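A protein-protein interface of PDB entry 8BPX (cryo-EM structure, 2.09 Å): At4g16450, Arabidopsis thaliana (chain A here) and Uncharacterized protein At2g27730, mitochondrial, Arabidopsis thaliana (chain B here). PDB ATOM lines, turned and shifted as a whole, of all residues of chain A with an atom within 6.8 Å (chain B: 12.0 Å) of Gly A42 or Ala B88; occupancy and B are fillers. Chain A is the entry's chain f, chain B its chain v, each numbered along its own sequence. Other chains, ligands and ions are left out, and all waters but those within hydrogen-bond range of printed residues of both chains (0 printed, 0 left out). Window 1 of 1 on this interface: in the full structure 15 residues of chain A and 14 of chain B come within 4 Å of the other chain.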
ATOM      1  N   PHE A  37      -3.216 -15.794   2.960  1.00  0.00           N
ATOM      2  CA  PHE A  37      -3.080 -17.120   3.547  1.00  0.00           C
ATOM      3  C   PHE A  37      -4.024 -17.299   4.733  1.00  0.00           C
ATOM      4  O   PHE A  37      -4.827 -18.244   4.781  1.00  0.00           O
ATOM      5  CB  PHE A  37      -1.613 -17.285   3.968  1.00  0.00           C
ATOM      6  CG  PHE A  37      -1.190 -18.692   4.265  1.00  0.00           C
ATOM      7  CD1 PHE A  37      -2.057 -19.755   4.115  1.00  0.00           C
ATOM      8  CD2 PHE A  37       0.107 -18.945   4.685  1.00  0.00           C
ATOM      9  CE1 PHE A  37      -1.647 -21.038   4.395  1.00  0.00           C
ATOM     10  CE2 PHE A  37       0.520 -20.225   4.962  1.00  0.00           C
ATOM     11  CZ  PHE A  37      -0.361 -21.275   4.817  1.00  0.00           C
ATOM     12  N   SER A  38      -3.957 -16.367   5.684  1.00  0.00           N
ATOM     13  CA  SER A  38      -4.746 -16.466   6.903  1.00  0.00           C
ATOM     14  C   SER A  38      -6.234 -16.342   6.612  1.00  0.00           C
ATOM     15  O   SER A  38      -7.043 -17.053   7.213  1.00  0.00           O
ATOM     16  CB  SER A  38      -4.300 -15.397   7.899  1.00  0.00           C
ATOM     17  OG  SER A  38      -4.823 -14.132   7.542  1.00  0.00           O
ATOM     18  N   THR A  39      -6.618 -15.450   5.696  1.00  0.00           N
ATOM     19  CA  THR A  39      -8.029 -15.294   5.359  1.00  0.00           C
ATOM     20  C   THR A  39      -8.593 -16.571   4.753  1.00  0.00           C
ATOM     21  O   THR A  39      -9.682 -17.025   5.133  1.00  0.00           O
ATOM     22  CB  THR A  39      -8.216 -14.121   4.393  1.00  0.00           C
ATOM     23  OG1 THR A  39      -7.784 -12.906   5.016  1.00  0.00           O
ATOM     24  CG2 THR A  39      -9.676 -13.989   3.983  1.00  0.00           C
ATOM     25  N   ILE A  40      -7.869 -17.163   3.801  1.00  0.00           N
ATOM     26  CA  ILE A  40      -8.362 -18.376   3.157  1.00  0.00           C
ATOM     27  C   ILE A  40      -8.488 -19.499   4.180  1.00  0.00           C
ATOM     28  O   ILE A  40      -9.512 -20.198   4.239  1.00  0.00           O
ATOM     29  CB  ILE A  40      -7.451 -18.757   1.974  1.00  0.00           C
ATOM     30  CG1 ILE A  40      -7.722 -17.826   0.788  1.00  0.00           C
ATOM     31  CG2 ILE A  40      -7.674 -20.204   1.555  1.00  0.00           C
ATOM     32  CD1 ILE A  40      -6.550 -17.663  -0.150  1.00  0.00           C
ATOM     33  N   THR A  41      -7.473 -19.659   5.036  1.00  0.00           N
ATOM     34  CA  THR A  41      -7.537 -20.695   6.064  1.00  0.00           C
ATOM     35  C   THR A  41      -8.690 -20.464   7.037  1.00  0.00           C
ATOM     36  O   THR A  41      -9.393 -21.413   7.410  1.00  0.00           O
ATOM     37  CB  THR A  41      -6.209 -20.772   6.812  1.00  0.00           C
ATOM     38  OG1 THR A  41      -5.132 -20.835   5.869  1.00  0.00           O
ATOM     39  CG2 THR A  41      -6.177 -21.990   7.727  1.00  0.00           C
ATOM     40  N   GLY A  42      -8.897 -19.218   7.469  1.00  0.00           N
ATOM     41  CA  GLY A  42      -9.961 -18.939   8.420  1.00  0.00           C
ATOM     42  C   GLY A  42     -11.341 -19.186   7.845  1.00  0.00           C
ATOM     43  O   GLY A  42     -12.202 -19.776   8.507  1.00  0.00           O
ATOM     44  N   ILE A  43     -11.571 -18.741   6.608  1.00  0.00           N
ATOM     45  CA  ILE A  43     -12.841 -19.018   5.944  1.00  0.00           C
ATOM     46  C   ILE A  43     -13.061 -20.520   5.833  1.00  0.00           C
ATOM     47  O   ILE A  43     -14.172 -21.020   6.057  1.00  0.00           O
ATOM     48  CB  ILE A  43     -12.882 -18.337   4.564  1.00  0.00           C
ATOM     49  CG1 ILE A  43     -12.992 -16.819   4.709  1.00  0.00           C
ATOM     50  CG2 ILE A  43     -14.038 -18.874   3.727  1.00  0.00           C
ATOM     51  CD1 ILE A  43     -12.701 -16.080   3.425  1.00  0.00           C
ATOM     52  N   SER A  44     -12.011 -21.263   5.478  1.00  0.00           N
ATOM     53  CA  SER A  44     -12.160 -22.704   5.318  1.00  0.00           C
ATOM     54  C   SER A  44     -12.496 -23.385   6.641  1.00  0.00           C
ATOM     55  O   SER A  44     -13.352 -24.277   6.684  1.00  0.00           O
ATOM     56  CB  SER A  44     -10.891 -23.286   4.706  1.00  0.00           C
ATOM     57  OG  SER A  44     -10.736 -22.848   3.369  1.00  0.00           O
ATOM     58  N   VAL A  45     -11.842 -22.971   7.730  1.00  0.00           N
ATOM     59  CA  VAL A  45     -12.155 -23.536   9.042  1.00  0.00           C
ATOM     60  C   VAL A  45     -13.595 -23.218   9.430  1.00  0.00           C
ATOM     61  O   VAL A  45     -14.309 -24.066   9.981  1.00  0.00           O
ATOM     62  CB  VAL A  45     -11.162 -23.030  10.105  1.00  0.00           C
ATOM     63  CG1 VAL A  45     -11.596 -23.474  11.493  1.00  0.00           C
ATOM     64  CG2 VAL A  45      -9.758 -23.527   9.811  1.00  0.00           C
ATOM     65  N   THR A  46     -14.039 -21.987   9.157  1.00  0.00           N
ATOM     66  CA  THR A  46     -15.408 -21.598   9.483  1.00  0.00           C
ATOM     67  C   THR A  46     -16.420 -22.449   8.721  1.00  0.00           C
ATOM     68  O   THR A  46     -17.415 -22.913   9.293  1.00  0.00           O
ATOM     69  CB  THR A  46     -15.610 -20.112   9.174  1.00  0.00           C
ATOM     70  OG1 THR A  46     -14.829 -19.324  10.083  1.00  0.00           O
ATOM     71  CG2 THR A  46     -17.078 -19.728   9.303  1.00  0.00           C
ATOM     72  N   VAL A  47     -16.180 -22.655   7.423  1.00  0.00           N
ATOM     73  CA  VAL A  47     -17.075 -23.485   6.623  1.00  0.00           C
ATOM     74  C   VAL A  47     -17.086 -24.913   7.153  1.00  0.00           C
ATOM     75  O   VAL A  47     -18.145 -25.541   7.262  1.00  0.00           O
ATOM     76  CB  VAL A  47     -16.681 -23.430   5.132  1.00  0.00           C
ATOM     77  CG1 VAL A  47     -17.481 -24.445   4.327  1.00  0.00           C
ATOM     78  CG2 VAL A  47     -16.900 -22.032   4.574  1.00  0.00           C
ATOM     79  N   MET A  62     -14.017 -29.147  11.028  1.00  0.00           N
ATOM     80  CA  MET A  62     -13.137 -27.989  11.110  1.00  0.00           C
ATOM     81  C   MET A  62     -11.723 -28.354  10.700  1.00  0.00           C
ATOM     82  O   MET A  62     -11.061 -27.592   9.992  1.00  0.00           O
ATOM     83  CB  MET A  62     -13.128 -27.425  12.528  1.00  0.00           C
ATOM     84  CG  MET A  62     -13.830 -26.110  12.682  1.00  0.00           C
ATOM     85  SD  MET A  62     -13.331 -25.279  14.201  1.00  0.00           S
ATOM     86  CE  MET A  62     -13.844 -26.499  15.399  1.00  0.00           C
ATOM     87  N   GLY A  69      -8.031 -25.408   3.467  1.00  0.00           N
ATOM     88  CA  GLY A  69      -7.709 -23.994   3.444  1.00  0.00           C
ATOM     89  C   GLY A  69      -6.225 -23.715   3.579  1.00  0.00           C
ATOM     90  O   GLY A  69      -5.703 -22.806   2.940  1.00  0.00           O
ATOM     91  N   ASP B  79     -17.222 -24.727  25.326  1.00  0.00           N
ATOM     92  CA  ASP B  79     -17.146 -25.522  24.103  1.00  0.00           C
ATOM     93  C   ASP B  79     -15.889 -25.102  23.347  1.00  0.00           C
ATOM     94  O   ASP B  79     -15.856 -24.051  22.702  1.00  0.00           O
ATOM     95  CB  ASP B  79     -18.411 -25.337  23.272  1.00  0.00           C
ATOM     96  CG  ASP B  79     -18.446 -26.211  22.031  1.00  0.00           C
ATOM     97  OD1 ASP B  79     -17.394 -26.730  21.605  1.00  0.00           O
ATOM     98  OD2 ASP B  79     -19.550 -26.381  21.473  1.00  0.00           O
ATOM     99  N   LYS B  80     -14.852 -25.938  23.429  1.00  0.00           N
ATOM    100  CA  LYS B  80     -13.549 -25.587  22.868  1.00  0.00           C
ATOM    101  C   LYS B  80     -13.611 -25.450  21.351  1.00  0.00           C
ATOM    102  O   LYS B  80     -13.055 -24.505  20.778  1.00  0.00           O
ATOM    103  CB  LYS B  80     -12.515 -26.638  23.273  1.00  0.00           C
ATOM    104  CG  LYS B  80     -11.648 -26.244  24.449  1.00  0.00           C
ATOM    105  CD  LYS B  80     -11.103 -27.474  25.163  1.00  0.00           C
ATOM    106  CE  LYS B  80     -10.874 -27.201  26.636  1.00  0.00           C
ATOM    107  NZ  LYS B  80      -9.924 -26.073  26.835  1.00  0.00           N
ATOM    108  N   ASN B  81     -14.280 -26.393  20.681  1.00  0.00           N
ATOM    109  CA  ASN B  81     -14.390 -26.329  19.226  1.00  0.00           C
ATOM    110  C   ASN B  81     -15.146 -25.080  18.785  1.00  0.00           C
ATOM    111  O   ASN B  81     -14.775 -24.438  17.795  1.00  0.00           O
ATOM    112  CB  ASN B  81     -15.071 -27.591  18.693  1.00  0.00           C
ATOM    113  CG  ASN B  81     -14.151 -28.794  18.689  1.00  0.00           C
ATOM    114  OD1 ASN B  81     -12.931 -28.662  18.764  1.00  0.00           O
ATOM    115  ND2 ASN B  81     -14.737 -29.979  18.604  1.00  0.00           N
ATOM    116  N   ARG B  82     -16.204 -24.716  19.514  1.00  0.00           N
ATOM    117  CA  ARG B  82     -16.921 -23.482  19.211  1.00  0.00           C
ATOM    118  C   ARG B  82     -16.011 -22.267  19.351  1.00  0.00           C
ATOM    119  O   ARG B  82     -16.042 -21.359  18.514  1.00  0.00           O
ATOM    120  CB  ARG B  82     -18.145 -23.340  20.118  1.00  0.00           C
ATOM    121  CG  ARG B  82     -19.077 -22.204  19.716  1.00  0.00           C
ATOM    122  CD  ARG B  82     -20.297 -22.105  20.627  1.00  0.00           C
ATOM    123  NE  ARG B  82     -19.936 -21.809  22.007  1.00  0.00           N
ATOM    124  CZ  ARG B  82     -20.352 -22.508  23.056  1.00  0.00           C
ATOM    125  NH1 ARG B  82     -21.167 -23.539  22.919  1.00  0.00           N
ATOM    126  NH2 ARG B  82     -19.936 -22.162  24.271  1.00  0.00           N
ATOM    127  N   ASN B  83     -15.194 -22.234  20.407  1.00  0.00           N
ATOM    128  CA  ASN B  83     -14.263 -21.126  20.600  1.00  0.00           C
ATOM    129  C   ASN B  83     -13.255 -21.041  19.461  1.00  0.00           C
ATOM    130  O   ASN B  83     -12.939 -19.945  18.977  1.00  0.00           O
ATOM    131  CB  ASN B  83     -13.543 -21.279  21.938  1.00  0.00           C
ATOM    132  CG  ASN B  83     -14.493 -21.231  23.120  1.00  0.00           C
ATOM    133  OD1 ASN B  83     -15.634 -20.783  22.998  1.00  0.00           O
ATOM    134  ND2 ASN B  83     -14.024 -21.683  24.273  1.00  0.00           N
ATOM    135  N   TYR B  84     -12.727 -22.189  19.030  1.00  0.00           N
ATOM    136  CA  TYR B  84     -11.789 -22.200  17.912  1.00  0.00           C
ATOM    137  C   TYR B  84     -12.453 -21.691  16.640  1.00  0.00           C
ATOM    138  O   TYR B  84     -11.850 -20.927  15.877  1.00  0.00           O
ATOM    139  CB  TYR B  84     -11.234 -23.610  17.704  1.00  0.00           C
ATOM    140  CG  TYR B  84     -10.461 -24.156  18.884  1.00  0.00           C
ATOM    141  CD1 TYR B  84      -9.906 -23.307  19.831  1.00  0.00           C
ATOM    142  CD2 TYR B  84     -10.303 -25.523  19.058  1.00  0.00           C
ATOM    143  CE1 TYR B  84      -9.208 -23.803  20.909  1.00  0.00           C
ATOM    144  CE2 TYR B  84      -9.607 -26.029  20.132  1.00  0.00           C
ATOM    145  CZ  TYR B  84      -9.061 -25.167  21.056  1.00  0.00           C
ATOM    146  OH  TYR B  84      -8.370 -25.666  22.130  1.00  0.00           O
ATOM    147  N   ALA B  85     -13.700 -22.104  16.397  1.00  0.00           N
ATOM    148  CA  ALA B  85     -14.428 -21.614  15.229  1.00  0.00           C
ATOM    149  C   ALA B  85     -14.645 -20.108  15.308  1.00  0.00           C
ATOM    150  O   ALA B  85     -14.584 -19.406  14.291  1.00  0.00           O
ATOM    151  CB  ALA B  85     -15.763 -22.343  15.102  1.00  0.00           C
ATOM    152  N   VAL B  86     -14.915 -19.598  16.510  1.00  0.00           N
ATOM    153  CA  VAL B  86     -15.062 -18.157  16.695  1.00  0.00           C
ATOM    154  C   VAL B  86     -13.763 -17.444  16.339  1.00  0.00           C
ATOM    155  O   VAL B  86     -13.767 -16.420  15.642  1.00  0.00           O
ATOM    156  CB  VAL B  86     -15.507 -17.853  18.137  1.00  0.00           C
ATOM    157  CG1 VAL B  86     -15.328 -16.390  18.452  1.00  0.00           C
ATOM    158  CG2 VAL B  86     -16.951 -18.271  18.338  1.00  0.00           C
ATOM    159  N   VAL B  87     -12.634 -17.981  16.803  1.00  0.00           N
ATOM    160  CA  VAL B  87     -11.338 -17.395  16.466  1.00  0.00           C
ATOM    161  C   VAL B  87     -11.120 -17.419  14.958  1.00  0.00           C
ATOM    162  O   VAL B  87     -10.616 -16.455  14.375  1.00  0.00           O
ATOM    163  CB  VAL B  87     -10.201 -18.115  17.213  1.00  0.00           C
ATOM    164  CG1 VAL B  87      -8.845 -17.609  16.734  1.00  0.00           C
ATOM    165  CG2 VAL B  87     -10.337 -17.911  18.709  1.00  0.00           C
ATOM    166  N   ALA B  88     -11.486 -18.524  14.306  1.00  0.00           N
ATOM    167  CA  ALA B  88     -11.305 -18.634  12.860  1.00  0.00           C
ATOM    168  C   ALA B  88     -12.146 -17.610  12.109  1.00  0.00           C
ATOM    169  O   ALA B  88     -11.675 -16.996  11.145  1.00  0.00           O
ATOM    170  CB  ALA B  88     -11.646 -20.046  12.390  1.00  0.00           C
ATOM    171  N   GLY B  89     -13.398 -17.422  12.526  1.00  0.00           N
ATOM    172  CA  GLY B  89     -14.228 -16.407  11.897  1.00  0.00           C
ATOM    173  C   GLY B  89     -13.682 -15.005  12.094  1.00  0.00           C
ATOM    174  O   GLY B  89     -13.685 -14.186  11.167  1.00  0.00           O
ATOM    175  N   VAL B  90     -13.193 -14.714  13.301  1.00  0.00           N
ATOM    176  CA  VAL B  90     -12.607 -13.403  13.568  1.00  0.00           C
ATOM    177  C   VAL B  90     -11.365 -13.193  12.711  1.00  0.00           C
ATOM    178  O   VAL B  90     -11.155 -12.112  12.150  1.00  0.00           O
ATOM    179  CB  VAL B  90     -12.291 -13.255  15.070  1.00  0.00           C
ATOM    180  CG1 VAL B  90     -11.305 -12.122  15.296  1.00  0.00           C
ATOM    181  CG2 VAL B  90     -13.567 -13.028  15.863  1.00  0.00           C
ATOM    182  N   VAL B  91     -10.522 -14.221  12.606  1.00  0.00           N
ATOM    183  CA  VAL B  91      -9.321 -14.127  11.784  1.00  0.00           C
ATOM    184  C   VAL B  91      -9.697 -13.898  10.329  1.00  0.00           C
ATOM    185  O   VAL B  91      -9.078 -13.086   9.640  1.00  0.00           O
ATOM    186  CB  VAL B  91      -8.447 -15.385  11.960  1.00  0.00           C
ATOM    187  CG1 VAL B  91      -7.470 -15.541  10.797  1.00  0.00           C
ATOM    188  CG2 VAL B  91      -7.691 -15.327  13.279  1.00  0.00           C
ATOM    189  N   ALA B  92     -10.732 -14.587   9.846  1.00  0.00           N
ATOM    190  CA  ALA B  92     -11.179 -14.380   8.471  1.00  0.00           C
ATOM    191  C   ALA B  92     -11.624 -12.938   8.249  1.00  0.00           C
ATOM    192  O   ALA B  92     -11.228 -12.300   7.269  1.00  0.00           O
ATOM    193  CB  ALA B  92     -12.308 -15.352   8.130  1.00  0.00           C
ATOM    194  N   ILE B  93     -12.427 -12.399   9.170  1.00  0.00           N
ATOM    195  CA  ILE B  93     -12.935 -11.035   9.011  1.00  0.00           C
ATOM    196  C   ILE B  93     -11.790 -10.025   9.024  1.00  0.00           C
ATOM    197  O   ILE B  93     -11.676  -9.169   8.134  1.00  0.00           O
ATOM    198  CB  ILE B  93     -13.972 -10.724  10.108  1.00  0.00           C
ATOM    199  CG1 ILE B  93     -15.327 -11.325   9.741  1.00  0.00           C
ATOM    200  CG2 ILE B  93     -14.097  -9.223  10.325  1.00  0.00           C
ATOM    201  CD1 ILE B  93     -16.093 -11.857  10.925  1.00  0.00           C
ATOM    202  N   VAL B  94     -10.918 -10.118  10.031  1.00  0.00           N
ATOM    203  CA  VAL B  94      -9.837  -9.149  10.177  1.00  0.00           C
ATOM    204  C   VAL B  94      -8.840  -9.276   9.031  1.00  0.00           C
ATOM    205  O   VAL B  94      -8.342  -8.271   8.508  1.00  0.00           O
ATOM    206  CB  VAL B  94      -9.148  -9.315  11.545  1.00  0.00           C
ATOM    207  CG1 VAL B  94      -8.008  -8.326  11.684  1.00  0.00           C
ATOM    208  CG2 VAL B  94     -10.149  -9.135  12.667  1.00  0.00           C
ATOM    209  N   GLY B  95      -8.522 -10.508   8.629  1.00  0.00           N
ATOM    210  CA  GLY B  95      -7.622 -10.702   7.513  1.00  0.00           C
ATOM    211  C   GLY B  95      -8.195 -10.193   6.209  1.00  0.00           C
ATOM    212  O   GLY B  95      -7.466  -9.678   5.367  1.00  0.00           O
ATOM    213  N   SER B  96      -9.511 -10.330   6.023  1.00  0.00           N
ATOM    214  CA  SER B  96     -10.149  -9.767   4.838  1.00  0.00           C
ATOM    215  C   SER B  96     -10.064  -8.247   4.837  1.00  0.00           C
ATOM    216  O   SER B  96      -9.808  -7.631   3.792  1.00  0.00           O
ATOM    217  CB  SER B  96     -11.608 -10.215   4.764  1.00  0.00           C
ATOM    218  OG  SER B  96     -11.732 -11.604   5.012  1.00  0.00           O
ATOM    219  N   ILE B  97     -10.284  -7.625   5.996  1.00  0.00           N
ATOM    220  CA  ILE B  97     -10.159  -6.171   6.080  1.00  0.00           C
ATOM    221  C   ILE B  97      -8.737  -5.744   5.739  1.00  0.00           C
ATOM    222  O   ILE B  97      -8.521  -4.820   4.949  1.00  0.00           O
ATOM    223  CB  ILE B  97     -10.583  -5.670   7.471  1.00  0.00           C
ATOM    224  CG1 ILE B  97     -12.103  -5.724   7.607  1.00  0.00           C
ATOM    225  CG2 ILE B  97     -10.079  -4.252   7.700  1.00  0.00           C
ATOM    226  CD1 ILE B  97     -12.568  -6.116   8.984  1.00  0.00           C
ATOM    227  N   TRP B  99      -6.566  -7.408   3.976  1.00  0.00           N
ATOM    228  CA  TRP B  99      -6.337  -7.723   2.572  1.00  0.00           C
ATOM    229  C   TRP B  99      -6.852  -6.607   1.678  1.00  0.00           C
ATOM    230  O   TRP B  99      -6.164  -6.174   0.746  1.00  0.00           O
ATOM    231  CB  TRP B  99      -7.015  -9.056   2.238  1.00  0.00           C
ATOM    232  CG  TRP B  99      -6.772  -9.613   0.859  1.00  0.00           C
ATOM    233  CD1 TRP B  99      -6.134  -9.005  -0.181  1.00  0.00           C
ATOM    234  CD2 TRP B  99      -7.174 -10.903   0.380  1.00  0.00           C
ATOM    235  NE1 TRP B  99      -6.116  -9.832  -1.277  1.00  0.00           N
ATOM    236  CE2 TRP B  99      -6.748 -11.004  -0.958  1.00  0.00           C
ATOM    237  CE3 TRP B  99      -7.859 -11.979   0.954  1.00  0.00           C
ATOM    238  CZ2 TRP B  99      -6.980 -12.140  -1.730  1.00  0.00           C
ATOM    239  CZ3 TRP B  99      -8.087 -13.106   0.184  1.00  0.00           C
ATOM    240  CH2 TRP B  99      -7.650 -13.177  -1.144  1.00  0.00           C
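Hydrophobic or aromatic side chains of chain A that line the printed part of chain B: Ile A43, Val A45 and Met A62.
Among the printed residues, no Asp or Glu carboxylate lies within 4 Å of a Lys or Arg side-chain nitrogen of the other chain.
The side-chain hydroxyl (OG1) of Thr A39 lies close to the backbone carbonyl oxygen (O) of Gly B95 (3.3 Å).
The backbone NH of Ser B96 sits at hydrogen-bond distance from the side-chain hydroxyl of Thr A39, 3.3 Å away.
The backbone NH (N) of Gly B89 sits at hydrogen-bond distance from the side-chain hydroxyl (OG1) of Thr A46, at 3.4 Å.
The backbone carbonyl oxygen (O) of Gly A42 is in hydrogen-bond range of the side-chain hydroxyl (OG1) of Thr A46 (3.1 Å).
The side-chain carboxylate (OD1) of Asp B79 lies within hydrogen-bond range of the backbone NH (N) of Asn B81 (3.3 Å).
The side-chain hydroxyl (OG) of Ser B96 lies within hydrogen-bond range of the backbone carbonyl oxygen (O) of Ala B92, 2.4 Å away.
O of Ser A38 touches CG1 of Val B91, 3.9 Å away.
CA of Gly A42 touches O of Ala B88, 3.8 Å away.
Ala B92 touches Gly A42.
Ile A43 touches Ala B92 (CG1 to CB, 3.8 Å).
Ala B88 touches Val A45.
Ala B88 touches Thr A46 (C to OG1, 3.8 Å).
Met A62 touches Asn B81.
SD of Met A62 touches N of Ala B85, at 3.9 Å.
Gly A42 touches just these residues of chain B: Ala B88 and Ala B92.
Of the printed residues of chain B, Ser A38 touches Val B91.
Of chain B, only Ala B92 comes within 4 Å of Ile A43.
Of chain B, only Ala B88 comes within 4 Å of Val A45.
Thr A46 touches just these residues of chain B: Ala B88 (3.8 Å) and Gly B89 (3.4 Å).
Printed residues of chain A within 4 Å of Val B91: Ser A38.
Of the printed residues of chain A, Gly B89 touches Thr A46.
The nearest residue of chain A that does not touch Ala B88 is Ile A43 (4.9 Å).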
